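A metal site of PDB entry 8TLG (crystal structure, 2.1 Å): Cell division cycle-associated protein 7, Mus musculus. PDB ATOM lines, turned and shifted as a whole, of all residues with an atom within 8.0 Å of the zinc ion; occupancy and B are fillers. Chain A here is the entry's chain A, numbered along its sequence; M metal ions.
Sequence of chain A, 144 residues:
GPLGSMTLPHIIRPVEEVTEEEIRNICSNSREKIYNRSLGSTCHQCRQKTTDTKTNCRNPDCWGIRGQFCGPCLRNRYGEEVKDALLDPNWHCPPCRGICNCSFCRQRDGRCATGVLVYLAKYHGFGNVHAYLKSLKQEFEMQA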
ATOM      1  N   HIS A  44     -16.704  13.316  13.934  1.00  0.00           N
ATOM      2  CA  HIS A  44     -16.671  14.002  12.647  1.00  0.00           C
ATOM      3  C   HIS A  44     -18.043  14.042  11.992  1.00  0.00           C
ATOM      4  O   HIS A  44     -18.383  15.026  11.318  1.00  0.00           O
ATOM      5  CB  HIS A  44     -15.672  13.311  11.711  1.00  0.00           C
ATOM      6  CG  HIS A  44     -15.737  13.783  10.296  1.00  0.00           C
ATOM      7  ND1 HIS A  44     -15.219  14.997   9.883  1.00  0.00           N
ATOM      8  CD2 HIS A  44     -16.271  13.206   9.187  1.00  0.00           C
ATOM      9  CE1 HIS A  44     -15.428  15.146   8.585  1.00  0.00           C
ATOM     10  NE2 HIS A  44     -16.062  14.077   8.137  1.00  0.00           N
ATOM     11  N   GLN A  45     -18.862  13.010  12.198  1.00  0.00           N
ATOM     12  CA  GLN A  45     -20.136  12.918  11.494  1.00  0.00           C
ATOM     13  C   GLN A  45     -21.152  13.901  12.076  1.00  0.00           C
ATOM     14  O   GLN A  45     -21.673  14.764  11.358  1.00  0.00           O
ATOM     15  CB  GLN A  45     -20.666  11.487  11.557  1.00  0.00           C
ATOM     16  CG  GLN A  45     -21.904  11.239  10.711  1.00  0.00           C
ATOM     17  CD  GLN A  45     -21.570  11.036   9.240  1.00  0.00           C
ATOM     18  OE1 GLN A  45     -20.432  10.727   8.882  1.00  0.00           O
ATOM     19  NE2 GLN A  45     -22.570  11.195   8.380  1.00  0.00           N
ATOM     20  N   ARG A  47     -20.578  16.041  14.712  1.00  0.00           N
ATOM     21  CA  ARG A  47     -19.925  17.278  15.141  1.00  0.00           C
ATOM     22  C   ARG A  47     -20.282  17.665  16.578  1.00  0.00           C
ATOM     23  O   ARG A  47     -20.348  18.846  16.922  1.00  0.00           O
ATOM     24  CB  ARG A  47     -20.224  18.419  14.171  1.00  0.00           C
ATOM     25  CG  ARG A  47     -19.855  18.086  12.731  1.00  0.00           C
ATOM     26  CD  ARG A  47     -19.886  19.292  11.810  1.00  0.00           C
ATOM     27  NE  ARG A  47     -21.243  19.684  11.425  1.00  0.00           N
ATOM     28  CZ  ARG A  47     -21.897  19.191  10.381  1.00  0.00           C
ATOM     29  NH1 ARG A  47     -21.367  18.242   9.616  1.00  0.00           N
ATOM     30  NH2 ARG A  47     -23.097  19.657  10.092  1.00  0.00           N
ATOM     31  N   ARG A  66     -10.869  13.980  11.852  1.00  0.00           N
ATOM     32  CA  ARG A  66     -11.705  13.449  10.786  1.00  0.00           C
ATOM     33  C   ARG A  66     -11.947  11.953  10.933  1.00  0.00           C
ATOM     34  O   ARG A  66     -12.922  11.437  10.366  1.00  0.00           O
ATOM     35  CB  ARG A  66     -11.071  13.749   9.422  1.00  0.00           C
ATOM     36  CG  ARG A  66      -9.866  12.883   9.099  1.00  0.00           C
ATOM     37  CD  ARG A  66      -8.898  13.574   8.149  1.00  0.00           C
ATOM     38  NE  ARG A  66      -9.415  13.673   6.789  1.00  0.00           N
ATOM     39  CZ  ARG A  66      -9.180  12.776   5.834  1.00  0.00           C
ATOM     40  NH1 ARG A  66      -8.469  11.685   6.066  1.00  0.00           N
ATOM     41  NH2 ARG A  66      -9.669  12.996   4.618  1.00  0.00           N
ATOM     42  N   PHE A  69     -15.353   8.889  15.135  1.00  0.00           N
ATOM     43  CA  PHE A  69     -16.778   8.675  14.934  1.00  0.00           C
ATOM     44  C   PHE A  69     -17.383   8.061  16.179  1.00  0.00           C
ATOM     45  O   PHE A  69     -16.799   7.154  16.779  1.00  0.00           O
ATOM     46  CB  PHE A  69     -17.036   7.771  13.714  1.00  0.00           C
ATOM     47  CG  PHE A  69     -16.769   8.444  12.395  1.00  0.00           C
ATOM     48  CD1 PHE A  69     -15.466   8.618  11.938  1.00  0.00           C
ATOM     49  CD2 PHE A  69     -17.811   8.915  11.614  1.00  0.00           C
ATOM     50  CE1 PHE A  69     -15.218   9.240  10.738  1.00  0.00           C
ATOM     51  CE2 PHE A  69     -17.566   9.533  10.405  1.00  0.00           C
ATOM     52  CZ  PHE A  69     -16.273   9.699   9.967  1.00  0.00           C
ATOM     53  N   TYR A  78     -22.679   4.058   8.489  1.00  0.00           N
ATOM     54  CA  TYR A  78     -21.772   3.169   7.770  1.00  0.00           C
ATOM     55  C   TYR A  78     -21.931   1.699   8.127  1.00  0.00           C
ATOM     56  O   TYR A  78     -21.194   0.867   7.582  1.00  0.00           O
ATOM     57  CB  TYR A  78     -20.318   3.593   7.999  1.00  0.00           C
ATOM     58  CG  TYR A  78     -20.080   5.061   7.706  1.00  0.00           C
ATOM     59  CD1 TYR A  78     -19.854   5.487   6.401  1.00  0.00           C
ATOM     60  CD2 TYR A  78     -20.108   6.008   8.714  1.00  0.00           C
ATOM     61  CE1 TYR A  78     -19.649   6.827   6.115  1.00  0.00           C
ATOM     62  CE2 TYR A  78     -19.906   7.346   8.442  1.00  0.00           C
ATOM     63  CZ  TYR A  78     -19.679   7.745   7.147  1.00  0.00           C
ATOM     64  OH  TYR A  78     -19.481   9.079   6.866  1.00  0.00           O
ATOM     65  N   PRO A  94     -13.980   6.602   7.343  1.00  0.00           N
ATOM     66  CA  PRO A  94     -14.685   6.819   6.080  1.00  0.00           C
ATOM     67  C   PRO A  94     -14.112   7.975   5.272  1.00  0.00           C
ATOM     68  O   PRO A  94     -14.033   7.877   4.042  1.00  0.00           O
ATOM     69  CB  PRO A  94     -16.130   7.105   6.534  1.00  0.00           C
ATOM     70  CG  PRO A  94     -16.261   6.352   7.815  1.00  0.00           C
ATOM     71  CD  PRO A  94     -14.903   6.439   8.480  1.00  0.00           C
ATOM     72  N   PRO A  95     -13.691   9.088   5.903  1.00  0.00           N
ATOM     73  CA  PRO A  95     -13.001  10.121   5.104  1.00  0.00           C
ATOM     74  C   PRO A  95     -11.752   9.601   4.407  1.00  0.00           C
ATOM     75  O   PRO A  95     -11.504   9.991   3.257  1.00  0.00           O
ATOM     76  CB  PRO A  95     -12.669  11.193   6.149  1.00  0.00           C
ATOM     77  CG  PRO A  95     -13.772  11.081   7.124  1.00  0.00           C
ATOM     78  CD  PRO A  95     -14.029   9.611   7.243  1.00  0.00           C
ATOM     79  N   ILE A  99     -15.564   7.614   1.495  1.00  0.00           N
ATOM     80  CA  ILE A  99     -16.959   7.225   1.538  1.00  0.00           C
ATOM     81  C   ILE A  99     -17.738   7.971   2.613  1.00  0.00           C
ATOM     82  O   ILE A  99     -18.852   7.568   2.960  1.00  0.00           O
ATOM     83  CB  ILE A  99     -17.094   5.696   1.729  1.00  0.00           C
ATOM     84  CG1 ILE A  99     -16.614   5.301   3.135  1.00  0.00           C
ATOM     85  CG2 ILE A  99     -16.312   4.940   0.669  1.00  0.00           C
ATOM     86  CD1 ILE A  99     -16.917   3.859   3.497  1.00  0.00           C
ATOM     87  N   CYS A 100     -17.178   9.045   3.154  1.00  0.00           N
ATOM     88  CA  CYS A 100     -17.863   9.782   4.198  1.00  0.00           C
ATOM     89  C   CYS A 100     -19.102  10.483   3.644  1.00  0.00           C
ATOM     90  O   CYS A 100     -19.018  11.182   2.629  1.00  0.00           O
ATOM     91  CB  CYS A 100     -16.933  10.802   4.846  1.00  0.00           C
ATOM     92  SG  CYS A 100     -17.631  11.600   6.326  1.00  0.00           S
ATOM     93  N   ASN A 101     -20.239  10.288   4.301  1.00  0.00           N
ATOM     94  CA  ASN A 101     -21.508  10.872   3.874  1.00  0.00           C
ATOM     95  C   ASN A 101     -22.013  11.954   4.814  1.00  0.00           C
ATOM     96  O   ASN A 101     -23.210  12.225   4.855  1.00  0.00           O
ATOM     97  CB  ASN A 101     -22.568   9.777   3.713  1.00  0.00           C
ATOM     98  CG  ASN A 101     -22.732   8.935   4.964  1.00  0.00           C
ATOM     99  OD1 ASN A 101     -23.143   9.435   6.008  1.00  0.00           O
ATOM    100  ND2 ASN A 101     -22.432   7.648   4.853  1.00  0.00           N
ATOM    101  N   CYS A 102     -21.108  12.584   5.575  1.00  0.00           N
ATOM    102  CA  CYS A 102     -21.516  13.696   6.411  1.00  0.00           C
ATOM    103  C   CYS A 102     -21.924  14.892   5.549  1.00  0.00           C
ATOM    104  O   CYS A 102     -21.660  14.932   4.344  1.00  0.00           O
ATOM    105  CB  CYS A 102     -20.391  14.093   7.373  1.00  0.00           C
ATOM    106  SG  CYS A 102     -19.080  15.099   6.614  1.00  0.00           S
ATOM    107  N   SER A 103     -22.573  15.869   6.185  1.00  0.00           N
ATOM    108  CA  SER A 103     -23.150  16.983   5.451  1.00  0.00           C
ATOM    109  C   SER A 103     -22.104  17.761   4.677  1.00  0.00           C
ATOM    110  O   SER A 103     -22.419  18.399   3.671  1.00  0.00           O
ATOM    111  CB  SER A 103     -23.897  17.917   6.402  1.00  0.00           C
ATOM    112  OG  SER A 103     -22.987  18.600   7.254  1.00  0.00           O
ATOM    113  N   PHE A 104     -20.847  17.736   5.128  1.00  0.00           N
ATOM    114  CA  PHE A 104     -19.783  18.468   4.446  1.00  0.00           C
ATOM    115  C   PHE A 104     -19.141  17.630   3.344  1.00  0.00           C
ATOM    116  O   PHE A 104     -18.930  18.126   2.232  1.00  0.00           O
ATOM    117  CB  PHE A 104     -18.727  18.914   5.457  1.00  0.00           C
ATOM    118  CG  PHE A 104     -17.515  19.544   4.832  1.00  0.00           C
ATOM    119  CD1 PHE A 104     -17.535  20.882   4.445  1.00  0.00           C
ATOM    120  CD2 PHE A 104     -16.358  18.821   4.639  1.00  0.00           C
ATOM    121  CE1 PHE A 104     -16.428  21.470   3.876  1.00  0.00           C
ATOM    122  CE2 PHE A 104     -15.238  19.407   4.065  1.00  0.00           C
ATOM    123  CZ  PHE A 104     -15.275  20.730   3.679  1.00  0.00           C
ATOM    124  N   CYS A 105     -18.826  16.373   3.626  1.00  0.00           N
ATOM    125  CA  CYS A 105     -18.062  15.552   2.691  1.00  0.00           C
ATOM    126  C   CYS A 105     -18.889  15.090   1.491  1.00  0.00           C
ATOM    127  O   CYS A 105     -18.304  14.756   0.452  1.00  0.00           O
ATOM    128  CB  CYS A 105     -17.466  14.345   3.399  1.00  0.00           C
ATOM    129  SG  CYS A 105     -16.126  14.727   4.552  1.00  0.00           S
ATOM    130  N   ARG A 106     -20.214  15.064   1.598  1.00  0.00           N
ATOM    131  CA  ARG A 106     -21.015  14.522   0.501  1.00  0.00           C
ATOM    132  C   ARG A 106     -21.326  15.561  -0.570  1.00  0.00           C
ATOM    133  O   ARG A 106     -21.456  15.199  -1.741  1.00  0.00           O
ATOM    134  CB  ARG A 106     -22.304  13.895   1.026  1.00  0.00           C
ATOM    135  CG  ARG A 106     -23.316  14.856   1.628  1.00  0.00           C
ATOM    136  CD  ARG A 106     -24.598  14.110   1.949  1.00  0.00           C
ATOM    137  NE  ARG A 106     -25.629  14.966   2.521  1.00  0.00           N
ATOM    138  CZ  ARG A 106     -25.978  14.960   3.799  1.00  0.00           C
ATOM    139  NH1 ARG A 106     -25.403  14.147   4.671  1.00  0.00           N
ATOM    140  NH2 ARG A 106     -26.947  15.782   4.203  1.00  0.00           N
HETATM  141 ZN    ZN M   1     -17.155  13.835   6.405  1.00  0.00          ZN
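SG of Cys 100 sits close to OH of Tyr 78, 3.2 Å away. The backbone NH (N) of Cys 100 is in hydrogen-bond range of the backbone carbonyl oxygen (O) of Pro 94, at 3.5 Å. The side-chain amide nitrogen (NE2) of Gln 45 sits close to the backbone NH (N) of Cys 102 (3.5 Å). The side-chain sulfur (SG) of Cys 102 lies close to the backbone NH (N) of Phe 104 (3.5 Å).
Within 4 Å of the zinc ion: His 44, Cys 100, Cys 102 and Cys 105.
NE2 of His 44 binds the zinc ion (2.1 Å). SG of Cys 100 binds the zinc ion (2.3 Å). The side-chain sulfur (SG) of Cys 105 binds the zinc ion (2.3 Å). SG of Cys 102 is bound to the zinc ion, 2.3 Å away. The zinc ion has four donor atoms within binding distance.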
